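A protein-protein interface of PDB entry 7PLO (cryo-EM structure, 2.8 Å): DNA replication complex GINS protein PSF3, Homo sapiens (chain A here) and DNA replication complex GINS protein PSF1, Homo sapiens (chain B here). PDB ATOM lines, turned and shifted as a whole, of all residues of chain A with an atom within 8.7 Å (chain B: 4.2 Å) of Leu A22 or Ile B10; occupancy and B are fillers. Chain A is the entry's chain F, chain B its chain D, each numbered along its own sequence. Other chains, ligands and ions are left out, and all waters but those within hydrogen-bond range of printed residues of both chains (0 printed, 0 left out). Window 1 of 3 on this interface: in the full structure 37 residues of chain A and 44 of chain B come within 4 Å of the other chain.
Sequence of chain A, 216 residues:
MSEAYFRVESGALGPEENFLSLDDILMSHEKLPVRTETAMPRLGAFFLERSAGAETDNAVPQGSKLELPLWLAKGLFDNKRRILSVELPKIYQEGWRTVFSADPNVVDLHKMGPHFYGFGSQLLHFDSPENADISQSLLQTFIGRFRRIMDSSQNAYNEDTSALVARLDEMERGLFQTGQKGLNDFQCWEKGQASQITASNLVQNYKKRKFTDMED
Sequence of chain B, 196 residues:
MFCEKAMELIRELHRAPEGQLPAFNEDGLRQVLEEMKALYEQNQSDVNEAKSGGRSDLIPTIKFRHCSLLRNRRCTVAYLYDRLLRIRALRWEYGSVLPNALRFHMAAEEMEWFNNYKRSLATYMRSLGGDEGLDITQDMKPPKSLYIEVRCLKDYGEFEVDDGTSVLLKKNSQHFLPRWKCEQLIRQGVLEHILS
SD of Met B7 lies close to ND1 of His A29 (3.7 Å).
A ring nitrogen (ND1) of His B14 sits at hydrogen-bond distance from the guanidinium group (NH1) of Arg A7, at 3.2 Å.
OD1 of Asp B82 is in hydrogen-bond range of OH of Tyr A5 (2.6 Å).
OE1 of Glu B8 lies within salt-bridge range of NH2 of Arg B11, at 2.8 Å.
The guanidinium group (NH1) of Arg A7 lies within salt-bridge range of the side-chain carboxylate (OD1) of Asp A23.
The side-chain hydroxyl of Ser A28 is in hydrogen-bond range of the backbone carbonyl oxygen of Ile A25, at 3.0 Å.
Leu A22 touches Ile B10 (CD2 to CD1, 3.7 Å).
OD2 of Asp B82 touches CD1 of Leu A22, 3.8 Å away.
CE of Met B7 touches CG2 of Ile A25, 3.7 Å away.
Cys B75 touches Ile A25.
Leu A26 touches Ile B10.
Leu A26 touches Arg B11 (CD2 to CG, 3.8 Å).
CD1 of Leu A26 touches CG of His B14 (3.4 Å).
Leu A22 touches just these residues of chain B: Ile B10 (3.7 Å) and Asp B82 (3.8 Å).
Ile B10 touches two residues of chain A.
Printed residues of chain A within 4 Å of His B14: Arg A7 (3.2 Å) and Leu A26 (3.4 Å).
Printed residues of chain B within 4 Å of His A29: Met B7 (3.5 Å).
Of the printed residues of chain B, Arg A7 touches His B14.
Printed residues of chain A within 4 Å of Arg B11: Leu A26 (3.8 Å).
The nearest residue of chain B that does not touch Leu A22 is Leu B13 (4.1 Å).
The nearest residue of chain A that does not touch Ile B10 is Ile A25 (4.03 Å).
The nearest printed residue of chain A that does not touch Arg B11 is His A29 (4.3 Å).
Hydrophobic or aromatic side chains of chain B within 4 Å of the printed part of chain A: Met B7, Ile B10 and His B14.
Along chain B the printed residues that touch a printed residue of chain A span positions 7 to 82.
Among the printed residues, no Asp or Glu carboxylate lies within 4 Å of a Lys or Arg side-chain nitrogen of the other chain.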
ATOM      1  N   TYR A   5      -6.130  25.291   9.413  1.00  0.00           N
ATOM      2  CA  TYR A   5      -5.729  23.911   9.648  1.00  0.00           C
ATOM      3  C   TYR A   5      -4.971  23.796  10.965  1.00  0.00           C
ATOM      4  O   TYR A   5      -4.077  24.599  11.250  1.00  0.00           O
ATOM      5  CB  TYR A   5      -4.858  23.413   8.494  1.00  0.00           C
ATOM      6  CG  TYR A   5      -3.981  22.229   8.829  1.00  0.00           C
ATOM      7  CD1 TYR A   5      -4.503  20.946   8.888  1.00  0.00           C
ATOM      8  CD2 TYR A   5      -2.624  22.394   9.069  1.00  0.00           C
ATOM      9  CE1 TYR A   5      -3.701  19.865   9.190  1.00  0.00           C
ATOM     10  CE2 TYR A   5      -1.818  21.322   9.372  1.00  0.00           C
ATOM     11  CZ  TYR A   5      -2.359  20.060   9.431  1.00  0.00           C
ATOM     12  OH  TYR A   5      -1.550  18.991   9.732  1.00  0.00           O
ATOM     13  N   ARG A   7      -3.265  20.410  13.140  1.00  0.00           N
ATOM     14  CA  ARG A   7      -3.041  18.980  13.256  1.00  0.00           C
ATOM     15  C   ARG A   7      -3.643  18.444  14.554  1.00  0.00           C
ATOM     16  O   ARG A   7      -4.036  19.195  15.451  1.00  0.00           O
ATOM     17  CB  ARG A   7      -1.545  18.667  13.205  1.00  0.00           C
ATOM     18  CG  ARG A   7      -0.701  19.406  14.242  1.00  0.00           C
ATOM     19  CD  ARG A   7       0.689  18.844  14.318  1.00  0.00           C
ATOM     20  NE  ARG A   7       1.419  18.981  13.064  1.00  0.00           N
ATOM     21  CZ  ARG A   7       2.641  18.509  12.851  1.00  0.00           C
ATOM     22  NH1 ARG A   7       3.302  17.841  13.783  1.00  0.00           N
ATOM     23  NH2 ARG A   7       3.215  18.713  11.669  1.00  0.00           N
ATOM     24  N   VAL A   8      -3.709  17.118  14.646  1.00  0.00           N
ATOM     25  CA  VAL A   8      -4.083  16.478  15.901  1.00  0.00           C
ATOM     26  C   VAL A   8      -2.997  16.763  16.928  1.00  0.00           C
ATOM     27  O   VAL A   8      -1.800  16.634  16.642  1.00  0.00           O
ATOM     28  CB  VAL A   8      -4.301  14.969  15.702  1.00  0.00           C
ATOM     29  CG1 VAL A   8      -4.631  14.277  17.031  1.00  0.00           C
ATOM     30  CG2 VAL A   8      -5.415  14.712  14.678  1.00  0.00           C
ATOM     31  N   GLU A   9      -3.412  17.152  18.127  1.00  0.00           N
ATOM     32  CA  GLU A   9      -2.477  17.559  19.161  1.00  0.00           C
ATOM     33  C   GLU A   9      -1.845  16.343  19.827  1.00  0.00           C
ATOM     34  O   GLU A   9      -2.447  15.271  19.916  1.00  0.00           O
ATOM     35  CB  GLU A   9      -3.181  18.420  20.213  1.00  0.00           C
ATOM     36  CG  GLU A   9      -3.802  19.716  19.675  1.00  0.00           C
ATOM     37  CD  GLU A   9      -5.190  19.531  19.073  1.00  0.00           C
ATOM     38  OE1 GLU A   9      -5.636  18.374  18.921  1.00  0.00           O
ATOM     39  OE2 GLU A   9      -5.831  20.550  18.744  1.00  0.00           O
ATOM     40  N   SER A  10      -0.611  16.520  20.290  1.00  0.00           N
ATOM     41  CA  SER A  10       0.106  15.441  20.954  1.00  0.00           C
ATOM     42  C   SER A  10      -0.509  15.123  22.311  1.00  0.00           C
ATOM     43  O   SER A  10      -0.876  16.023  23.070  1.00  0.00           O
ATOM     44  CB  SER A  10       1.577  15.813  21.123  1.00  0.00           C
ATOM     45  OG  SER A  10       2.242  14.890  21.965  1.00  0.00           O
ATOM     46  N   GLY A  11      -0.625  13.827  22.601  1.00  0.00           N
ATOM     47  CA  GLY A  11      -1.061  13.333  23.896  1.00  0.00           C
ATOM     48  C   GLY A  11       0.023  12.596  24.659  1.00  0.00           C
ATOM     49  O   GLY A  11      -0.279  11.821  25.571  1.00  0.00           O
ATOM     50  N   GLU A  17      -0.731   8.094  24.467  1.00  0.00           N
ATOM     51  CA  GLU A  17      -0.533   9.034  23.378  1.00  0.00           C
ATOM     52  C   GLU A  17      -1.721   9.009  22.421  1.00  0.00           C
ATOM     53  O   GLU A  17      -2.471   8.033  22.342  1.00  0.00           O
ATOM     54  CB  GLU A  17       0.767   8.720  22.638  1.00  0.00           C
ATOM     55  CG  GLU A  17       0.729   7.477  21.760  1.00  0.00           C
ATOM     56  CD  GLU A  17       2.111   7.032  21.332  1.00  0.00           C
ATOM     57  OE1 GLU A  17       2.954   6.774  22.215  1.00  0.00           O
ATOM     58  OE2 GLU A  17       2.357   6.948  20.112  1.00  0.00           O
ATOM     59  N   ASN A  18      -1.885  10.106  21.688  1.00  0.00           N
ATOM     60  CA  ASN A  18      -2.995  10.219  20.752  1.00  0.00           C
ATOM     61  C   ASN A  18      -2.751   9.353  19.524  1.00  0.00           C
ATOM     62  O   ASN A  18      -1.665   9.367  18.939  1.00  0.00           O
ATOM     63  CB  ASN A  18      -3.205  11.677  20.347  1.00  0.00           C
ATOM     64  CG  ASN A  18      -3.915  12.488  21.417  1.00  0.00           C
ATOM     65  OD1 ASN A  18      -4.413  11.947  22.405  1.00  0.00           O
ATOM     66  ND2 ASN A  18      -3.978  13.794  21.215  1.00  0.00           N
ATOM     67  N   PHE A  19      -3.787   8.605  19.140  1.00  0.00           N
ATOM     68  CA  PHE A  19      -3.677   7.631  18.059  1.00  0.00           C
ATOM     69  C   PHE A  19      -3.333   8.296  16.733  1.00  0.00           C
ATOM     70  O   PHE A  19      -2.486   7.800  15.982  1.00  0.00           O
ATOM     71  CB  PHE A  19      -4.995   6.863  17.963  1.00  0.00           C
ATOM     72  CG  PHE A  19      -5.001   5.764  16.948  1.00  0.00           C
ATOM     73  CD1 PHE A  19      -4.532   4.506  17.274  1.00  0.00           C
ATOM     74  CD2 PHE A  19      -5.510   5.977  15.681  1.00  0.00           C
ATOM     75  CE1 PHE A  19      -4.551   3.489  16.348  1.00  0.00           C
ATOM     76  CE2 PHE A  19      -5.529   4.965  14.752  1.00  0.00           C
ATOM     77  CZ  PHE A  19      -5.053   3.718  15.087  1.00  0.00           C
ATOM     78  N   LEU A  20      -3.973   9.422  16.432  1.00  0.00           N
ATOM     79  CA  LEU A  20      -3.837  10.094  15.147  1.00  0.00           C
ATOM     80  C   LEU A  20      -2.745  11.158  15.128  1.00  0.00           C
ATOM     81  O   LEU A  20      -2.591  11.840  14.110  1.00  0.00           O
ATOM     82  CB  LEU A  20      -5.176  10.731  14.755  1.00  0.00           C
ATOM     83  CG  LEU A  20      -6.347   9.762  14.566  1.00  0.00           C
ATOM     84  CD1 LEU A  20      -7.663  10.509  14.514  1.00  0.00           C
ATOM     85  CD2 LEU A  20      -6.172   8.938  13.311  1.00  0.00           C
ATOM     86  N   SER A  21      -1.983  11.319  16.210  1.00  0.00           N
ATOM     87  CA  SER A  21      -0.989  12.381  16.289  1.00  0.00           C
ATOM     88  C   SER A  21       0.294  11.970  15.576  1.00  0.00           C
ATOM     89  O   SER A  21       0.941  10.983  15.950  1.00  0.00           O
ATOM     90  CB  SER A  21      -0.697  12.734  17.744  1.00  0.00           C
ATOM     91  OG  SER A  21       0.420  13.599  17.822  1.00  0.00           O
ATOM     92  N   LEU A  22       0.668  12.752  14.560  1.00  0.00           N
ATOM     93  CA  LEU A  22       1.923  12.520  13.853  1.00  0.00           C
ATOM     94  C   LEU A  22       3.115  12.687  14.786  1.00  0.00           C
ATOM     95  O   LEU A  22       4.100  11.944  14.685  1.00  0.00           O
ATOM     96  CB  LEU A  22       2.038  13.480  12.668  1.00  0.00           C
ATOM     97  CG  LEU A  22       0.876  13.538  11.670  1.00  0.00           C
ATOM     98  CD1 LEU A  22       1.150  14.595  10.622  1.00  0.00           C
ATOM     99  CD2 LEU A  22       0.637  12.196  11.011  1.00  0.00           C
ATOM    100  N   ASP A  23       3.050  13.669  15.691  1.00  0.00           N
ATOM    101  CA  ASP A  23       4.126  13.865  16.658  1.00  0.00           C
ATOM    102  C   ASP A  23       4.294  12.643  17.547  1.00  0.00           C
ATOM    103  O   ASP A  23       5.419  12.207  17.807  1.00  0.00           O
ATOM    104  CB  ASP A  23       3.851  15.100  17.514  1.00  0.00           C
ATOM    105  CG  ASP A  23       3.735  16.365  16.696  1.00  0.00           C
ATOM    106  OD1 ASP A  23       2.660  16.590  16.102  1.00  0.00           O
ATOM    107  OD2 ASP A  23       4.717  17.134  16.643  1.00  0.00           O
ATOM    108  N   ASP A  24       3.184  12.075  18.019  1.00  0.00           N
ATOM    109  CA  ASP A  24       3.263  10.893  18.869  1.00  0.00           C
ATOM    110  C   ASP A  24       3.777   9.687  18.096  1.00  0.00           C
ATOM    111  O   ASP A  24       4.518   8.866  18.643  1.00  0.00           O
ATOM    112  CB  ASP A  24       1.896  10.592  19.474  1.00  0.00           C
ATOM    113  CG  ASP A  24       1.416  11.691  20.396  1.00  0.00           C
ATOM    114  OD1 ASP A  24       2.186  12.641  20.642  1.00  0.00           O
ATOM    115  OD2 ASP A  24       0.268  11.606  20.879  1.00  0.00           O
ATOM    116  N   ILE A  25       3.388   9.558  16.827  1.00  0.00           N
ATOM    117  CA  ILE A  25       3.874   8.447  16.009  1.00  0.00           C
ATOM    118  C   ILE A  25       5.389   8.548  15.827  1.00  0.00           C
ATOM    119  O   ILE A  25       6.132   7.573  16.031  1.00  0.00           O
ATOM    120  CB  ILE A  25       3.117   8.421  14.665  1.00  0.00           C
ATOM    121  CG1 ILE A  25       1.668   7.963  14.892  1.00  0.00           C
ATOM    122  CG2 ILE A  25       3.793   7.507  13.662  1.00  0.00           C
ATOM    123  CD1 ILE A  25       0.695   8.350  13.796  1.00  0.00           C
ATOM    124  N   LEU A  26       5.870   9.742  15.470  1.00  0.00           N
ATOM    125  CA  LEU A  26       7.307   9.949  15.306  1.00  0.00           C
ATOM    126  C   LEU A  26       8.052   9.746  16.619  1.00  0.00           C
ATOM    127  O   LEU A  26       9.158   9.195  16.635  1.00  0.00           O
ATOM    128  CB  LEU A  26       7.568  11.350  14.754  1.00  0.00           C
ATOM    129  CG  LEU A  26       7.158  11.608  13.301  1.00  0.00           C
ATOM    130  CD1 LEU A  26       7.213  13.091  12.994  1.00  0.00           C
ATOM    131  CD2 LEU A  26       8.044  10.843  12.330  1.00  0.00           C
ATOM    132  N   MET A  27       7.464  10.191  17.730  1.00  0.00           N
ATOM    133  CA  MET A  27       8.078  10.005  19.039  1.00  0.00           C
ATOM    134  C   MET A  27       8.193   8.526  19.389  1.00  0.00           C
ATOM    135  O   MET A  27       9.243   8.064  19.847  1.00  0.00           O
ATOM    136  CB  MET A  27       7.254  10.768  20.079  1.00  0.00           C
ATOM    137  CG  MET A  27       7.607  10.530  21.553  1.00  0.00           C
ATOM    138  SD  MET A  27       6.829   9.110  22.373  1.00  0.00           S
ATOM    139  CE  MET A  27       5.080   9.410  22.114  1.00  0.00           C
ATOM    140  N   SER A  28       7.119   7.763  19.174  1.00  0.00           N
ATOM    141  CA  SER A  28       7.121   6.345  19.507  1.00  0.00           C
ATOM    142  C   SER A  28       7.963   5.512  18.550  1.00  0.00           C
ATOM    143  O   SER A  28       8.227   4.344  18.849  1.00  0.00           O
ATOM    144  CB  SER A  28       5.688   5.807  19.537  1.00  0.00           C
ATOM    145  OG  SER A  28       4.977   6.156  18.363  1.00  0.00           O
ATOM    146  N   HIS A  29       8.380   6.067  17.408  1.00  0.00           N
ATOM    147  CA  HIS A  29       9.322   5.341  16.559  1.00  0.00           C
ATOM    148  C   HIS A  29      10.727   5.251  17.161  1.00  0.00           C
ATOM    149  O   HIS A  29      11.507   4.391  16.741  1.00  0.00           O
ATOM    150  CB  HIS A  29       9.411   5.993  15.181  1.00  0.00           C
ATOM    151  CG  HIS A  29      10.121   5.153  14.164  1.00  0.00           C
ATOM    152  ND1 HIS A  29       9.738   3.864  13.866  1.00  0.00           N
ATOM    153  CD2 HIS A  29      11.195   5.415  13.384  1.00  0.00           C
ATOM    154  CE1 HIS A  29      10.541   3.369  12.943  1.00  0.00           C
ATOM    155  NE2 HIS A  29      11.436   4.290  12.633  1.00  0.00           N
ATOM    156  N   HIS A 115      11.850  14.779  20.925  1.00  0.00           N
ATOM    157  CA  HIS A 115      10.668  14.636  21.787  1.00  0.00           C
ATOM    158  C   HIS A 115      11.052  14.168  23.194  1.00  0.00           C
ATOM    159  O   HIS A 115      10.647  13.088  23.648  1.00  0.00           O
ATOM    160  CB  HIS A 115       9.679  13.660  21.160  1.00  0.00           C
ATOM    161  CG  HIS A 115       9.195  14.066  19.805  1.00  0.00           C
ATOM    162  ND1 HIS A 115       9.848  13.713  18.644  1.00  0.00           N
ATOM    163  CD2 HIS A 115       8.111  14.782  19.425  1.00  0.00           C
ATOM    164  CE1 HIS A 115       9.189  14.200  17.607  1.00  0.00           C
ATOM    165  NE2 HIS A 115       8.132  14.853  18.054  1.00  0.00           N
ATOM    166  N   ALA B   6       6.126   2.637   6.647  1.00  0.00           N
ATOM    167  CA  ALA B   6       5.030   3.430   7.188  1.00  0.00           C
ATOM    168  C   ALA B   6       5.495   4.813   7.624  1.00  0.00           C
ATOM    169  O   ALA B   6       4.722   5.776   7.564  1.00  0.00           O
ATOM    170  CB  ALA B   6       4.396   2.686   8.360  1.00  0.00           C
ATOM    171  N   MET B   7       6.750   4.935   8.064  1.00  0.00           N
ATOM    172  CA  MET B   7       7.246   6.216   8.551  1.00  0.00           C
ATOM    173  C   MET B   7       7.420   7.237   7.435  1.00  0.00           C
ATOM    174  O   MET B   7       7.430   8.439   7.712  1.00  0.00           O
ATOM    175  CB  MET B   7       8.581   6.031   9.269  1.00  0.00           C
ATOM    176  CG  MET B   7       8.519   5.287  10.585  1.00  0.00           C
ATOM    177  SD  MET B   7       7.628   6.177  11.866  1.00  0.00           S
ATOM    178  CE  MET B   7       6.078   5.297  11.806  1.00  0.00           C
ATOM    179  N   GLU B   8       7.603   6.795   6.188  1.00  0.00           N
ATOM    180  CA  GLU B   8       7.831   7.745   5.102  1.00  0.00           C
ATOM    181  C   GLU B   8       6.611   8.628   4.875  1.00  0.00           C
ATOM    182  O   GLU B   8       6.742   9.843   4.681  1.00  0.00           O
ATOM    183  CB  GLU B   8       8.196   6.996   3.819  1.00  0.00           C
ATOM    184  CG  GLU B   8       9.434   6.106   3.921  1.00  0.00           C
ATOM    185  CD  GLU B   8      10.700   6.874   4.259  1.00  0.00           C
ATOM    186  OE1 GLU B   8      10.847   7.308   5.421  1.00  0.00           O
ATOM    187  OE2 GLU B   8      11.549   7.046   3.359  1.00  0.00           O
ATOM    188  N   LEU B   9       5.419   8.031   4.906  1.00  0.00           N
ATOM    189  CA  LEU B   9       4.173   8.787   4.809  1.00  0.00           C
ATOM    190  C   LEU B   9       4.074   9.836   5.916  1.00  0.00           C
ATOM    191  O   LEU B   9       3.797  11.023   5.665  1.00  0.00           O
ATOM    192  CB  LEU B   9       3.004   7.803   4.900  1.00  0.00           C
ATOM    193  CG  LEU B   9       2.897   6.680   3.869  1.00  0.00           C
ATOM    194  CD1 LEU B   9       1.793   5.712   4.257  1.00  0.00           C
ATOM    195  CD2 LEU B   9       2.631   7.243   2.500  1.00  0.00           C
ATOM    196  N   ILE B  10       4.312   9.400   7.155  1.00  0.00           N
ATOM    197  CA  ILE B  10       4.199  10.271   8.318  1.00  0.00           C
ATOM    198  C   ILE B  10       5.200  11.412   8.227  1.00  0.00           C
ATOM    199  O   ILE B  10       4.872  12.564   8.522  1.00  0.00           O
ATOM    200  CB  ILE B  10       4.396   9.448   9.608  1.00  0.00           C
ATOM    201  CG1 ILE B  10       3.321   8.355   9.755  1.00  0.00           C
ATOM    202  CG2 ILE B  10       4.434  10.355  10.834  1.00  0.00           C
ATOM    203  CD1 ILE B  10       1.886   8.845   9.914  1.00  0.00           C
ATOM    204  N   ARG B  11       6.438  11.106   7.838  1.00  0.00           N
ATOM    205  CA  ARG B  11       7.460  12.140   7.738  1.00  0.00           C
ATOM    206  C   ARG B  11       7.145  13.122   6.619  1.00  0.00           C
ATOM    207  O   ARG B  11       7.387  14.327   6.763  1.00  0.00           O
ATOM    208  CB  ARG B  11       8.831  11.503   7.525  1.00  0.00           C
ATOM    209  CG  ARG B  11       9.418  10.880   8.789  1.00  0.00           C
ATOM    210  CD  ARG B  11      10.886  10.495   8.623  1.00  0.00           C
ATOM    211  NE  ARG B  11      11.060   9.144   8.088  1.00  0.00           N
ATOM    212  CZ  ARG B  11      11.386   8.055   8.781  1.00  0.00           C
ATOM    213  NH1 ARG B  11      11.580   8.083  10.092  1.00  0.00           N
ATOM    214  NH2 ARG B  11      11.515   6.899   8.140  1.00  0.00           N
ATOM    215  N   GLU B  12       6.607  12.624   5.498  1.00  0.00           N
ATOM    216  CA  GLU B  12       6.191  13.502   4.409  1.00  0.00           C
ATOM    217  C   GLU B  12       5.172  14.522   4.890  1.00  0.00           C
ATOM    218  O   GLU B  12       5.286  15.716   4.595  1.00  0.00           O
ATOM    219  CB  GLU B  12       5.604  12.677   3.262  1.00  0.00           C
ATOM    220  CG  GLU B  12       6.631  12.063   2.332  1.00  0.00           C
ATOM    221  CD  GLU B  12       6.004  11.142   1.303  1.00  0.00           C
ATOM    222  OE1 GLU B  12       4.762  11.010   1.297  1.00  0.00           O
ATOM    223  OE2 GLU B  12       6.754  10.549   0.499  1.00  0.00           O
ATOM    224  N   LEU B  13       4.168  14.070   5.646  1.00  0.00           N
ATOM    225  CA  LEU B  13       3.178  15.025   6.142  1.00  0.00           C
ATOM    226  C   LEU B  13       3.751  15.925   7.234  1.00  0.00           C
ATOM    227  O   LEU B  13       3.456  17.125   7.267  1.00  0.00           O
ATOM    228  CB  LEU B  13       1.936  14.297   6.652  1.00  0.00           C
ATOM    229  CG  LEU B  13       0.996  13.644   5.634  1.00  0.00           C
ATOM    230  CD1 LEU B  13      -0.233  13.186   6.363  1.00  0.00           C
ATOM    231  CD2 LEU B  13       0.585  14.554   4.483  1.00  0.00           C
ATOM    232  N   HIS B  14       4.561  15.370   8.139  1.00  0.00           N
ATOM    233  CA  HIS B  14       5.063  16.151   9.266  1.00  0.00           C
ATOM    234  C   HIS B  14       6.000  17.262   8.811  1.00  0.00           C
ATOM    235  O   HIS B  14       5.982  18.361   9.378  1.00  0.00           O
ATOM    236  CB  HIS B  14       5.777  15.242  10.263  1.00  0.00           C
ATOM    237  CG  HIS B  14       6.558  15.989  11.297  1.00  0.00           C
ATOM    238  ND1 HIS B  14       5.961  16.642  12.351  1.00  0.00           N
ATOM    239  CD2 HIS B  14       7.889  16.201  11.430  1.00  0.00           C
ATOM    240  CE1 HIS B  14       6.889  17.218  13.095  1.00  0.00           C
ATOM    241  NE2 HIS B  14       8.067  16.965  12.557  1.00  0.00           N
ATOM    242  N   CYS B  75      -0.385   4.074  11.383  1.00  0.00           N
ATOM    243  CA  CYS B  75       0.284   5.041  10.519  1.00  0.00           C
ATOM    244  C   CYS B  75      -0.561   5.369   9.294  1.00  0.00           C
ATOM    245  O   CYS B  75      -0.687   6.543   8.915  1.00  0.00           O
ATOM    246  CB  CYS B  75       1.648   4.507  10.101  1.00  0.00           C
ATOM    247  SG  CYS B  75       2.828   4.375  11.452  1.00  0.00           S
ATOM    248  N   ASP B  82      -4.880  13.131   8.532  1.00  0.00           N
ATOM    249  CA  ASP B  82      -4.270  14.457   8.476  1.00  0.00           C
ATOM    250  C   ASP B  82      -4.430  15.076   7.090  1.00  0.00           C
ATOM    251  O   ASP B  82      -4.627  16.298   6.962  1.00  0.00           O
ATOM    252  CB  ASP B  82      -2.801  14.374   8.876  1.00  0.00           C
ATOM    253  CG  ASP B  82      -2.128  15.733   8.914  1.00  0.00           C
ATOM    254  OD1 ASP B  82      -2.437  16.522   9.831  1.00  0.00           O
ATOM    255  OD2 ASP B  82      -1.292  16.018   8.034  1.00  0.00           O
